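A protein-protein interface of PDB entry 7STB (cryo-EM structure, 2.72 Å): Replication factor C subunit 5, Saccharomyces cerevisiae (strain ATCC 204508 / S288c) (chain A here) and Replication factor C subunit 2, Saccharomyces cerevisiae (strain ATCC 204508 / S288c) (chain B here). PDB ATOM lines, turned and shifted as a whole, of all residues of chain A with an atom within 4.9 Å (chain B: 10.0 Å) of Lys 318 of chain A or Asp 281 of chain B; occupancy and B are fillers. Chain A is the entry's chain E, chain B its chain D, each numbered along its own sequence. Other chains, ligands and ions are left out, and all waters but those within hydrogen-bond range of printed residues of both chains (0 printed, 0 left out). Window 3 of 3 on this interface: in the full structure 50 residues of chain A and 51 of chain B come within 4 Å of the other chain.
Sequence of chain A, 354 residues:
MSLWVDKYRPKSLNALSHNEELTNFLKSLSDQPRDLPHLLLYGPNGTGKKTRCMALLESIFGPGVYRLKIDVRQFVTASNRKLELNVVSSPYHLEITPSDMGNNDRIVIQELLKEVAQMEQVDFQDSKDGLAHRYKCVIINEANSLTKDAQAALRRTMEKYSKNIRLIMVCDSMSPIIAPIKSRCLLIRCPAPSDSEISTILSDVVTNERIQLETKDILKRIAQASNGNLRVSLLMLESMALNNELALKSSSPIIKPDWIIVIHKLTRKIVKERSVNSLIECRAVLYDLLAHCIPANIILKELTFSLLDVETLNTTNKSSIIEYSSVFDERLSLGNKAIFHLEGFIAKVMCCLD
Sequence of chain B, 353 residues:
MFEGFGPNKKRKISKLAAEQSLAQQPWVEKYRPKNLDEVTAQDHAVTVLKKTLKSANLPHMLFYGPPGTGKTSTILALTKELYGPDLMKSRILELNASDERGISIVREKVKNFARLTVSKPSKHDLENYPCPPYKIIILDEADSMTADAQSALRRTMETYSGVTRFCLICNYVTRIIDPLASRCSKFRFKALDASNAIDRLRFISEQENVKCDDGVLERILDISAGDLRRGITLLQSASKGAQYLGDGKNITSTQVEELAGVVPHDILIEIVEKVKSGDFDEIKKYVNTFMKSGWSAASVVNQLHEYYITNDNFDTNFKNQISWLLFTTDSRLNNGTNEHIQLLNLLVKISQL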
ATOM      1  N   LEU A 308     -11.677   7.467  -3.345  1.00  0.00           N
ATOM      2  CA  LEU A 308     -10.851   8.533  -2.791  1.00  0.00           C
ATOM      3  C   LEU A 308      -9.854   8.033  -1.753  1.00  0.00           C
ATOM      4  O   LEU A 308      -8.935   8.778  -1.399  1.00  0.00           O
ATOM      5  CB  LEU A 308     -11.738   9.611  -2.166  1.00  0.00           C
ATOM      6  CG  LEU A 308     -12.526  10.497  -3.133  1.00  0.00           C
ATOM      7  CD1 LEU A 308     -13.371  11.500  -2.362  1.00  0.00           C
ATOM      8  CD2 LEU A 308     -11.599  11.210  -4.104  1.00  0.00           C
ATOM      9  N   VAL A 310      -7.901   5.372  -2.240  1.00  0.00           N
ATOM     10  CA  VAL A 310      -6.822   4.652  -2.906  1.00  0.00           C
ATOM     11  C   VAL A 310      -5.541   5.470  -2.821  1.00  0.00           C
ATOM     12  O   VAL A 310      -5.526   6.668  -3.129  1.00  0.00           O
ATOM     13  CB  VAL A 310      -7.199   4.353  -4.364  1.00  0.00           C
ATOM     14  CG1 VAL A 310      -6.035   3.699  -5.093  1.00  0.00           C
ATOM     15  CG2 VAL A 310      -8.437   3.466  -4.420  1.00  0.00           C
ATOM     16  N   LEU A 313      -3.736   6.850  -6.416  1.00  0.00           N
ATOM     17  CA  LEU A 313      -4.217   8.061  -7.064  1.00  0.00           C
ATOM     18  C   LEU A 313      -3.583   9.301  -6.442  1.00  0.00           C
ATOM     19  O   LEU A 313      -3.224   9.320  -5.261  1.00  0.00           O
ATOM     20  CB  LEU A 313      -5.739   8.149  -6.961  1.00  0.00           C
ATOM     21  CG  LEU A 313      -6.510   6.903  -7.403  1.00  0.00           C
ATOM     22  CD1 LEU A 313      -8.000   7.189  -7.459  1.00  0.00           C
ATOM     23  CD2 LEU A 313      -6.005   6.407  -8.747  1.00  0.00           C
ATOM     24  N   ASN A 314      -3.447  10.345  -7.257  1.00  0.00           N
ATOM     25  CA  ASN A 314      -2.864  11.606  -6.831  1.00  0.00           C
ATOM     26  C   ASN A 314      -3.967  12.636  -6.592  1.00  0.00           C
ATOM     27  O   ASN A 314      -5.162  12.346  -6.691  1.00  0.00           O
ATOM     28  CB  ASN A 314      -1.853  12.103  -7.868  1.00  0.00           C
ATOM     29  CG  ASN A 314      -2.418  12.124  -9.275  1.00  0.00           C
ATOM     30  OD1 ASN A 314      -3.608  12.366  -9.476  1.00  0.00           O
ATOM     31  ND2 ASN A 314      -1.562  11.872 -10.259  1.00  0.00           N
ATOM     32  N   THR A 315      -3.553  13.865  -6.273  1.00  0.00           N
ATOM     33  CA  THR A 315      -4.515  14.905  -5.923  1.00  0.00           C
ATOM     34  C   THR A 315      -5.444  15.224  -7.090  1.00  0.00           C
ATOM     35  O   THR A 315      -6.654  15.390  -6.900  1.00  0.00           O
ATOM     36  CB  THR A 315      -3.779  16.167  -5.471  1.00  0.00           C
ATOM     37  OG1 THR A 315      -2.707  15.810  -4.589  1.00  0.00           O
ATOM     38  CG2 THR A 315      -4.729  17.113  -4.749  1.00  0.00           C
ATOM     39  N   THR A 316      -4.896  15.324  -8.302  1.00  0.00           N
ATOM     40  CA  THR A 316      -5.721  15.667  -9.457  1.00  0.00           C
ATOM     41  C   THR A 316      -6.784  14.605  -9.711  1.00  0.00           C
ATOM     42  O   THR A 316      -7.946  14.929  -9.988  1.00  0.00           O
ATOM     43  CB  THR A 316      -4.839  15.846 -10.694  1.00  0.00           C
ATOM     44  OG1 THR A 316      -4.032  17.019 -10.544  1.00  0.00           O
ATOM     45  CG2 THR A 316      -5.690  15.975 -11.951  1.00  0.00           C
ATOM     46  N   ASN A 317      -6.402  13.329  -9.626  1.00  0.00           N
ATOM     47  CA  ASN A 317      -7.365  12.258  -9.847  1.00  0.00           C
ATOM     48  C   ASN A 317      -8.487  12.313  -8.819  1.00  0.00           C
ATOM     49  O   ASN A 317      -9.663  12.161  -9.165  1.00  0.00           O
ATOM     50  CB  ASN A 317      -6.659  10.902  -9.797  1.00  0.00           C
ATOM     51  CG  ASN A 317      -5.902  10.592 -11.073  1.00  0.00           C
ATOM     52  OD1 ASN A 317      -6.424  10.760 -12.175  1.00  0.00           O
ATOM     53  ND2 ASN A 317      -4.662  10.137 -10.932  1.00  0.00           N
ATOM     54  N   LYS A 318      -8.143  12.538  -7.550  1.00  0.00           N
ATOM     55  CA  LYS A 318      -9.159  12.608  -6.506  1.00  0.00           C
ATOM     56  C   LYS A 318     -10.079  13.809  -6.702  1.00  0.00           C
ATOM     57  O   LYS A 318     -11.296  13.707  -6.502  1.00  0.00           O
ATOM     58  CB  LYS A 318      -8.485  12.659  -5.135  1.00  0.00           C
ATOM     59  CG  LYS A 318      -7.827  11.350  -4.730  1.00  0.00           C
ATOM     60  CD  LYS A 318      -6.762  11.563  -3.669  1.00  0.00           C
ATOM     61  CE  LYS A 318      -6.164  10.243  -3.215  1.00  0.00           C
ATOM     62  NZ  LYS A 318      -4.979  10.436  -2.335  1.00  0.00           N
ATOM     63  N   SER A 319      -9.515  14.958  -7.084  1.00  0.00           N
ATOM     64  CA  SER A 319     -10.340  16.136  -7.331  1.00  0.00           C
ATOM     65  C   SER A 319     -11.314  15.892  -8.475  1.00  0.00           C
ATOM     66  O   SER A 319     -12.501  16.231  -8.380  1.00  0.00           O
ATOM     67  CB  SER A 319      -9.452  17.341  -7.635  1.00  0.00           C
ATOM     68  OG  SER A 319      -8.594  17.631  -6.546  1.00  0.00           O
ATOM     69  N   SER A 320     -10.831  15.297  -9.565  1.00  0.00           N
ATOM     70  CA  SER A 320     -11.723  14.974 -10.672  1.00  0.00           C
ATOM     71  C   SER A 320     -12.787  13.975 -10.239  1.00  0.00           C
ATOM     72  O   SER A 320     -13.951  14.078 -10.647  1.00  0.00           O
ATOM     73  CB  SER A 320     -10.917  14.426 -11.846  1.00  0.00           C
ATOM     74  OG  SER A 320      -9.942  15.359 -12.274  1.00  0.00           O
ATOM     75  N   ILE A 321     -12.405  12.999  -9.413  1.00  0.00           N
ATOM     76  CA  ILE A 321     -13.359  11.995  -8.953  1.00  0.00           C
ATOM     77  C   ILE A 321     -14.479  12.655  -8.161  1.00  0.00           C
ATOM     78  O   ILE A 321     -15.661  12.362  -8.367  1.00  0.00           O
ATOM     79  CB  ILE A 321     -12.639  10.917  -8.122  1.00  0.00           C
ATOM     80  CG1 ILE A 321     -11.801  10.018  -9.031  1.00  0.00           C
ATOM     81  CG2 ILE A 321     -13.645  10.082  -7.341  1.00  0.00           C
ATOM     82  CD1 ILE A 321     -10.707   9.266  -8.306  1.00  0.00           C
ATOM     83  N   ILE A 322     -14.126  13.558  -7.244  1.00  0.00           N
ATOM     84  CA  ILE A 322     -15.150  14.197  -6.422  1.00  0.00           C
ATOM     85  C   ILE A 322     -16.017  15.124  -7.269  1.00  0.00           C
ATOM     86  O   ILE A 322     -17.234  15.218  -7.061  1.00  0.00           O
ATOM     87  CB  ILE A 322     -14.509  14.933  -5.227  1.00  0.00           C
ATOM     88  CG1 ILE A 322     -15.586  15.436  -4.259  1.00  0.00           C
ATOM     89  CG2 ILE A 322     -13.637  16.085  -5.688  1.00  0.00           C
ATOM     90  CD1 ILE A 322     -16.329  14.335  -3.539  1.00  0.00           C
ATOM     91  N   LYS B 274      -8.298  24.470   6.838  1.00  0.00           N
ATOM     92  CA  LYS B 274      -8.086  23.250   6.064  1.00  0.00           C
ATOM     93  C   LYS B 274      -8.115  23.535   4.568  1.00  0.00           C
ATOM     94  O   LYS B 274      -7.293  23.005   3.811  1.00  0.00           O
ATOM     95  CB  LYS B 274      -9.141  22.204   6.428  1.00  0.00           C
ATOM     96  CG  LYS B 274      -9.063  21.706   7.864  1.00  0.00           C
ATOM     97  CD  LYS B 274      -7.826  20.853   8.096  1.00  0.00           C
ATOM     98  CE  LYS B 274      -7.800  20.293   9.508  1.00  0.00           C
ATOM     99  NZ  LYS B 274      -6.559  19.519   9.783  1.00  0.00           N
ATOM    100  N   SER B 277      -4.820  25.307   3.316  1.00  0.00           N
ATOM    101  CA  SER B 277      -3.732  24.339   3.182  1.00  0.00           C
ATOM    102  C   SER B 277      -4.230  23.201   2.301  1.00  0.00           C
ATOM    103  O   SER B 277      -4.744  22.189   2.782  1.00  0.00           O
ATOM    104  CB  SER B 277      -3.281  23.839   4.549  1.00  0.00           C
ATOM    105  OG  SER B 277      -3.042  24.920   5.433  1.00  0.00           O
ATOM    106  N   GLY B 278      -4.074  23.372   0.991  1.00  0.00           N
ATOM    107  CA  GLY B 278      -4.579  22.408   0.034  1.00  0.00           C
ATOM    108  C   GLY B 278      -4.042  21.008   0.245  1.00  0.00           C
ATOM    109  O   GLY B 278      -2.859  20.743   0.011  1.00  0.00           O
ATOM    110  N   ASP B 279      -4.910  20.103   0.689  1.00  0.00           N
ATOM    111  CA  ASP B 279      -4.535  18.707   0.890  1.00  0.00           C
ATOM    112  C   ASP B 279      -5.805  17.875   0.840  1.00  0.00           C
ATOM    113  O   ASP B 279      -6.667  18.015   1.712  1.00  0.00           O
ATOM    114  CB  ASP B 279      -3.810  18.517   2.223  1.00  0.00           C
ATOM    115  CG  ASP B 279      -3.393  17.079   2.464  1.00  0.00           C
ATOM    116  OD1 ASP B 279      -3.599  16.237   1.565  1.00  0.00           O
ATOM    117  OD2 ASP B 279      -2.857  16.790   3.554  1.00  0.00           O
ATOM    118  N   PHE B 280      -5.923  17.017  -0.175  1.00  0.00           N
ATOM    119  CA  PHE B 280      -7.151  16.250  -0.347  1.00  0.00           C
ATOM    120  C   PHE B 280      -7.398  15.319   0.833  1.00  0.00           C
ATOM    121  O   PHE B 280      -8.532  15.199   1.308  1.00  0.00           O
ATOM    122  CB  PHE B 280      -7.098  15.455  -1.651  1.00  0.00           C
ATOM    123  CG  PHE B 280      -8.451  15.124  -2.208  1.00  0.00           C
ATOM    124  CD1 PHE B 280      -9.225  14.131  -1.635  1.00  0.00           C
ATOM    125  CD2 PHE B 280      -8.953  15.809  -3.300  1.00  0.00           C
ATOM    126  CE1 PHE B 280     -10.472  13.825  -2.142  1.00  0.00           C
ATOM    127  CE2 PHE B 280     -10.199  15.506  -3.811  1.00  0.00           C
ATOM    128  CZ  PHE B 280     -10.959  14.513  -3.232  1.00  0.00           C
ATOM    129  N   ASP B 281      -6.353  14.647   1.318  1.00  0.00           N
ATOM    130  CA  ASP B 281      -6.533  13.695   2.410  1.00  0.00           C
ATOM    131  C   ASP B 281      -6.997  14.398   3.681  1.00  0.00           C
ATOM    132  O   ASP B 281      -7.991  13.997   4.302  1.00  0.00           O
ATOM    133  CB  ASP B 281      -5.231  12.935   2.660  1.00  0.00           C
ATOM    134  CG  ASP B 281      -4.835  12.055   1.491  1.00  0.00           C
ATOM    135  OD1 ASP B 281      -5.737  11.603   0.753  1.00  0.00           O
ATOM    136  OD2 ASP B 281      -3.623  11.813   1.309  1.00  0.00           O
ATOM    137  N   GLU B 282      -6.289  15.454   4.083  1.00  0.00           N
ATOM    138  CA  GLU B 282      -6.667  16.176   5.293  1.00  0.00           C
ATOM    139  C   GLU B 282      -8.050  16.797   5.149  1.00  0.00           C
ATOM    140  O   GLU B 282      -8.867  16.742   6.077  1.00  0.00           O
ATOM    141  CB  GLU B 282      -5.628  17.250   5.606  1.00  0.00           C
ATOM    142  CG  GLU B 282      -4.331  16.710   6.187  1.00  0.00           C
ATOM    143  CD  GLU B 282      -4.486  16.224   7.614  1.00  0.00           C
ATOM    144  OE1 GLU B 282      -5.212  16.879   8.392  1.00  0.00           O
ATOM    145  OE2 GLU B 282      -3.881  15.187   7.960  1.00  0.00           O
ATOM    146  N   ILE B 283      -8.329  17.392   3.988  1.00  0.00           N
ATOM    147  CA  ILE B 283      -9.615  18.050   3.781  1.00  0.00           C
ATOM    148  C   ILE B 283     -10.747  17.035   3.865  1.00  0.00           C
ATOM    149  O   ILE B 283     -11.766  17.273   4.519  1.00  0.00           O
ATOM    150  CB  ILE B 283      -9.624  18.800   2.436  1.00  0.00           C
ATOM    151  CG1 ILE B 283      -8.802  20.086   2.548  1.00  0.00           C
ATOM    152  CG2 ILE B 283     -11.054  19.111   2.007  1.00  0.00           C
ATOM    153  CD1 ILE B 283      -8.543  20.774   1.224  1.00  0.00           C
ATOM    154  N   LYS B 284     -10.586  15.885   3.205  1.00  0.00           N
ATOM    155  CA  LYS B 284     -11.650  14.885   3.217  1.00  0.00           C
ATOM    156  C   LYS B 284     -11.831  14.290   4.609  1.00  0.00           C
ATOM    157  O   LYS B 284     -12.963  14.033   5.034  1.00  0.00           O
ATOM    158  CB  LYS B 284     -11.368  13.792   2.184  1.00  0.00           C
ATOM    159  CG  LYS B 284     -10.267  12.815   2.559  1.00  0.00           C
ATOM    160  CD  LYS B 284     -10.024  11.798   1.454  1.00  0.00           C
ATOM    161  CE  LYS B 284     -11.098  10.719   1.424  1.00  0.00           C
ATOM    162  NZ  LYS B 284     -11.018   9.808   2.597  1.00  0.00           N
ATOM    163  N   LYS B 285     -10.735  14.066   5.338  1.00  0.00           N
ATOM    164  CA  LYS B 285     -10.858  13.558   6.702  1.00  0.00           C
ATOM    165  C   LYS B 285     -11.619  14.543   7.583  1.00  0.00           C
ATOM    166  O   LYS B 285     -12.545  14.160   8.316  1.00  0.00           O
ATOM    167  CB  LYS B 285      -9.469  13.278   7.278  1.00  0.00           C
ATOM    168  CG  LYS B 285      -9.480  12.743   8.702  1.00  0.00           C
ATOM    169  CD  LYS B 285      -8.076  12.408   9.177  1.00  0.00           C
ATOM    170  CE  LYS B 285      -8.090  11.816  10.577  1.00  0.00           C
ATOM    171  NZ  LYS B 285      -8.463  12.824  11.607  1.00  0.00           N
ATOM    172  N   TYR B 286     -11.248  15.825   7.520  1.00  0.00           N
ATOM    173  CA  TYR B 286     -11.931  16.819   8.338  1.00  0.00           C
ATOM    174  C   TYR B 286     -13.390  16.955   7.926  1.00  0.00           C
ATOM    175  O   TYR B 286     -14.264  17.156   8.775  1.00  0.00           O
ATOM    176  CB  TYR B 286     -11.226  18.171   8.242  1.00  0.00           C
ATOM    177  CG  TYR B 286     -11.803  19.201   9.187  1.00  0.00           C
ATOM    178  CD1 TYR B 286     -11.288  19.365  10.465  1.00  0.00           C
ATOM    179  CD2 TYR B 286     -12.876  19.996   8.809  1.00  0.00           C
ATOM    180  CE1 TYR B 286     -11.816  20.298  11.335  1.00  0.00           C
ATOM    181  CE2 TYR B 286     -13.411  20.930   9.672  1.00  0.00           C
ATOM    182  CZ  TYR B 286     -12.878  21.077  10.933  1.00  0.00           C
ATOM    183  OH  TYR B 286     -13.410  22.007  11.796  1.00  0.00           O
ATOM    184  N   VAL B 287     -13.673  16.860   6.626  1.00  0.00           N
ATOM    185  CA  VAL B 287     -15.049  16.962   6.159  1.00  0.00           C
ATOM    186  C   VAL B 287     -15.872  15.788   6.669  1.00  0.00           C
ATOM    187  O   VAL B 287     -17.029  15.953   7.064  1.00  0.00           O
ATOM    188  CB  VAL B 287     -15.084  17.058   4.624  1.00  0.00           C
ATOM    189  CG1 VAL B 287     -16.488  16.817   4.102  1.00  0.00           C
ATOM    190  CG2 VAL B 287     -14.583  18.413   4.174  1.00  0.00           C
ATOM    191  N   ASN B 288     -15.298  14.584   6.655  1.00  0.00           N
ATOM    192  CA  ASN B 288     -16.005  13.428   7.196  1.00  0.00           C
ATOM    193  C   ASN B 288     -16.303  13.623   8.677  1.00  0.00           C
ATOM    194  O   ASN B 288     -17.429  13.385   9.138  1.00  0.00           O
ATOM    195  CB  ASN B 288     -15.176  12.161   6.975  1.00  0.00           C
ATOM    196  CG  ASN B 288     -15.997  10.896   7.110  1.00  0.00           C
ATOM    197  OD1 ASN B 288     -17.226  10.943   7.178  1.00  0.00           O
ATOM    198  ND2 ASN B 288     -15.321   9.755   7.157  1.00  0.00           N
ATOM    199  N   THR B 289     -15.304  14.078   9.438  1.00  0.00           N
ATOM    200  CA  THR B 289     -15.519  14.305  10.863  1.00  0.00           C
ATOM    201  C   THR B 289     -16.597  15.358  11.097  1.00  0.00           C
ATOM    202  O   THR B 289     -17.454  15.196  11.974  1.00  0.00           O
ATOM    203  CB  THR B 289     -14.208  14.723  11.530  1.00  0.00           C
ATOM    204  OG1 THR B 289     -13.222  13.701  11.334  1.00  0.00           O
ATOM    205  CG2 THR B 289     -14.410  14.945  13.022  1.00  0.00           C
ATOM    206  N   ILE B 341     -21.052  14.934  -0.188  1.00  0.00           N
ATOM    207  CA  ILE B 341     -20.317  15.024  -1.448  1.00  0.00           C
ATOM    208  C   ILE B 341     -20.222  16.473  -1.905  1.00  0.00           C
ATOM    209  O   ILE B 341     -19.159  16.945  -2.329  1.00  0.00           O
ATOM    210  CB  ILE B 341     -20.988  14.144  -2.518  1.00  0.00           C
ATOM    211  CG1 ILE B 341     -20.843  12.663  -2.161  1.00  0.00           C
ATOM    212  CG2 ILE B 341     -20.391  14.428  -3.889  1.00  0.00           C
ATOM    213  CD1 ILE B 341     -21.717  11.746  -2.994  1.00  0.00           C
ATOM    214  N   LEU B 344     -17.768  18.467   0.243  1.00  0.00           N
ATOM    215  CA  LEU B 344     -16.383  18.112  -0.047  1.00  0.00           C
ATOM    216  C   LEU B 344     -15.934  18.711  -1.375  1.00  0.00           C
ATOM    217  O   LEU B 344     -14.821  19.244  -1.480  1.00  0.00           O
ATOM    218  CB  LEU B 344     -16.220  16.591  -0.054  1.00  0.00           C
ATOM    219  CG  LEU B 344     -14.809  16.060  -0.317  1.00  0.00           C
ATOM    220  CD1 LEU B 344     -13.816  16.641   0.677  1.00  0.00           C
ATOM    221  CD2 LEU B 344     -14.796  14.545  -0.256  1.00  0.00           C
ATOM    222  N   ASN B 345     -16.787  18.639  -2.401  1.00  0.00           N
ATOM    223  CA  ASN B 345     -16.428  19.217  -3.693  1.00  0.00           C
ATOM    224  C   ASN B 345     -16.241  20.724  -3.592  1.00  0.00           C
ATOM    225  O   ASN B 345     -15.300  21.276  -4.171  1.00  0.00           O
ATOM    226  CB  ASN B 345     -17.490  18.898  -4.742  1.00  0.00           C
ATOM    227  CG  ASN B 345     -17.060  19.302  -6.139  1.00  0.00           C
ATOM    228  OD1 ASN B 345     -15.973  19.845  -6.331  1.00  0.00           O
ATOM    229  ND2 ASN B 345     -17.922  19.066  -7.117  1.00  0.00           N
ATOM    230  N   VAL B 348     -12.902  21.434  -1.832  1.00  0.00           N
ATOM    231  CA  VAL B 348     -11.771  21.133  -2.707  1.00  0.00           C
ATOM    232  C   VAL B 348     -11.638  22.195  -3.793  1.00  0.00           C
ATOM    233  O   VAL B 348     -10.530  22.651  -4.102  1.00  0.00           O
ATOM    234  CB  VAL B 348     -11.923  19.724  -3.309  1.00  0.00           C
ATOM    235  CG1 VAL B 348     -10.933  19.520  -4.445  1.00  0.00           C
ATOM    236  CG2 VAL B 348     -11.727  18.667  -2.234  1.00  0.00           C
ATOM    237  N   LYS B 349     -12.760  22.600  -4.392  1.00  0.00           N
ATOM    238  CA  LYS B 349     -12.709  23.589  -5.462  1.00  0.00           C
ATOM    239  C   LYS B 349     -12.185  24.926  -4.955  1.00  0.00           C
ATOM    240  O   LYS B 349     -11.379  25.577  -5.628  1.00  0.00           O
ATOM    241  CB  LYS B 349     -14.092  23.752  -6.091  1.00  0.00           C
ATOM    242  CG  LYS B 349     -14.393  22.723  -7.170  1.00  0.00           C
ATOM    243  CD  LYS B 349     -15.875  22.660  -7.492  1.00  0.00           C
ATOM    244  CE  LYS B 349     -16.134  21.896  -8.780  1.00  0.00           C
ATOM    245  NZ  LYS B 349     -15.609  22.616  -9.972  1.00  0.00           N
ATOM    246  N   SER B 351     -10.205  25.242  -2.451  1.00  0.00           N
ATOM    247  CA  SER B 351      -8.792  24.999  -2.178  1.00  0.00           C
ATOM    248  C   SER B 351      -7.959  25.148  -3.444  1.00  0.00           C
ATOM    249  O   SER B 351      -6.852  25.701  -3.408  1.00  0.00           O
ATOM    250  CB  SER B 351      -8.608  23.608  -1.575  1.00  0.00           C
ATOM    251  OG  SER B 351      -8.944  22.600  -2.511  1.00  0.00           O
ATOM    252  N   GLN B 352      -8.472  24.656  -4.574  1.00  0.00           N
ATOM    253  CA  GLN B 352      -7.737  24.771  -5.830  1.00  0.00           C
ATOM    254  C   GLN B 352      -7.509  26.228  -6.209  1.00  0.00           C
ATOM    255  O   GLN B 352      -6.409  26.601  -6.634  1.00  0.00           O
ATOM    256  CB  GLN B 352      -8.488  24.044  -6.943  1.00  0.00           C
ATOM    257  CG  GLN B 352      -8.555  22.539  -6.768  1.00  0.00           C
ATOM    258  CD  GLN B 352      -9.326  21.861  -7.880  1.00  0.00           C
ATOM    259  OE1 GLN B 352      -9.874  22.521  -8.764  1.00  0.00           O
ATOM    260  NE2 GLN B 352      -9.370  20.537  -7.845  1.00  0.00           N
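Among the printed residues, merely in contact across the chains: Lys 318 of chain A with Phe 280 of chain B, Ser 319 of chain A with Phe 280 of chain B, Leu 308 of chain A with Phe 280 of chain B, Ile 322 of chain A with Leu 344 of chain B, Ser 319 of chain A with Val 348 of chain B, Leu 308 of chain A with Lys 284 of chain B, Ile 322 of chain A with Asn 345 of chain B, Ile 322 of chain A with Phe 280 of chain B and Leu 308 of chain A with Leu 344 of chain B.
O of Thr 315 of chain A sits at hydrogen-bond distance from OG of Ser 319 of chain A (3.0 Å). The side-chain carboxylate (OD1) of Asp 279 of chain B is in hydrogen-bond range of the backbone NH (N) of Asp 281 of chain B (3.2 Å).
Leu 308 of chain A touches three residues of chain B. Leu 313 of chain A touches none of the printed residues of chain B. Of chain B, only Phe 280 and Asp 281 come within 4 Å of Lys 318 of chain A. Ser 319 of chain A touches just these residues of chain B: Phe 280 (3.4 Å), Val 348 (3.7 Å) and Gln 352 (3.2 Å). No residue of chain B comes within 4 Å of Ser 320 of chain A. Gly 278 of chain B touches none of the printed residues of chain A. Printed residues of chain A within 4 Å of Asp 281 of chain B: Lys 318. Of the printed residues of chain A, Leu 344 of chain B touches Leu 308 and Ile 322. Of the printed residues of chain A, Asn 345 of chain B touches Ile 322 (3.9 Å). Of the printed residues of chain A, Val 348 of chain B touches Ser 319. The nearest residue of chain B that does not touch Lys 318 of chain A is Lys 284 of chain B (6.1 Å). The nearest printed residue of chain A that does not touch Lys 284 of chain B is Lys 318 of chain A (6.1 Å).
Of the 12 printed residues of chain A, 4 touch a printed residue of chain B. Printed residues of chain A that touch a printed residue of chain B: Leu 308, Lys 318, Ser 319 and Ile 322. Hydrophobic or aromatic side chains of chain B within 4 Å of the printed part of chain A: Phe 280, Leu 344 and Val 348. Among the printed residues, 11 pairs touch across the chains. Among the printed residues, Asp or Glu carboxylates within 4 Å of a Lys or Arg side-chain nitrogen of the other chain: Lys 318 of chain A with Asp 281 of chain B (3.4 Å).
OG of Ser 319 of chain A lies close to NE2 of Gln 352 of chain B (3.3 Å). The side-chain amino group of Lys 318 of chain A is in salt-bridge range of the side-chain carboxylate of Asp 281 of chain B, at 3.4 Å.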
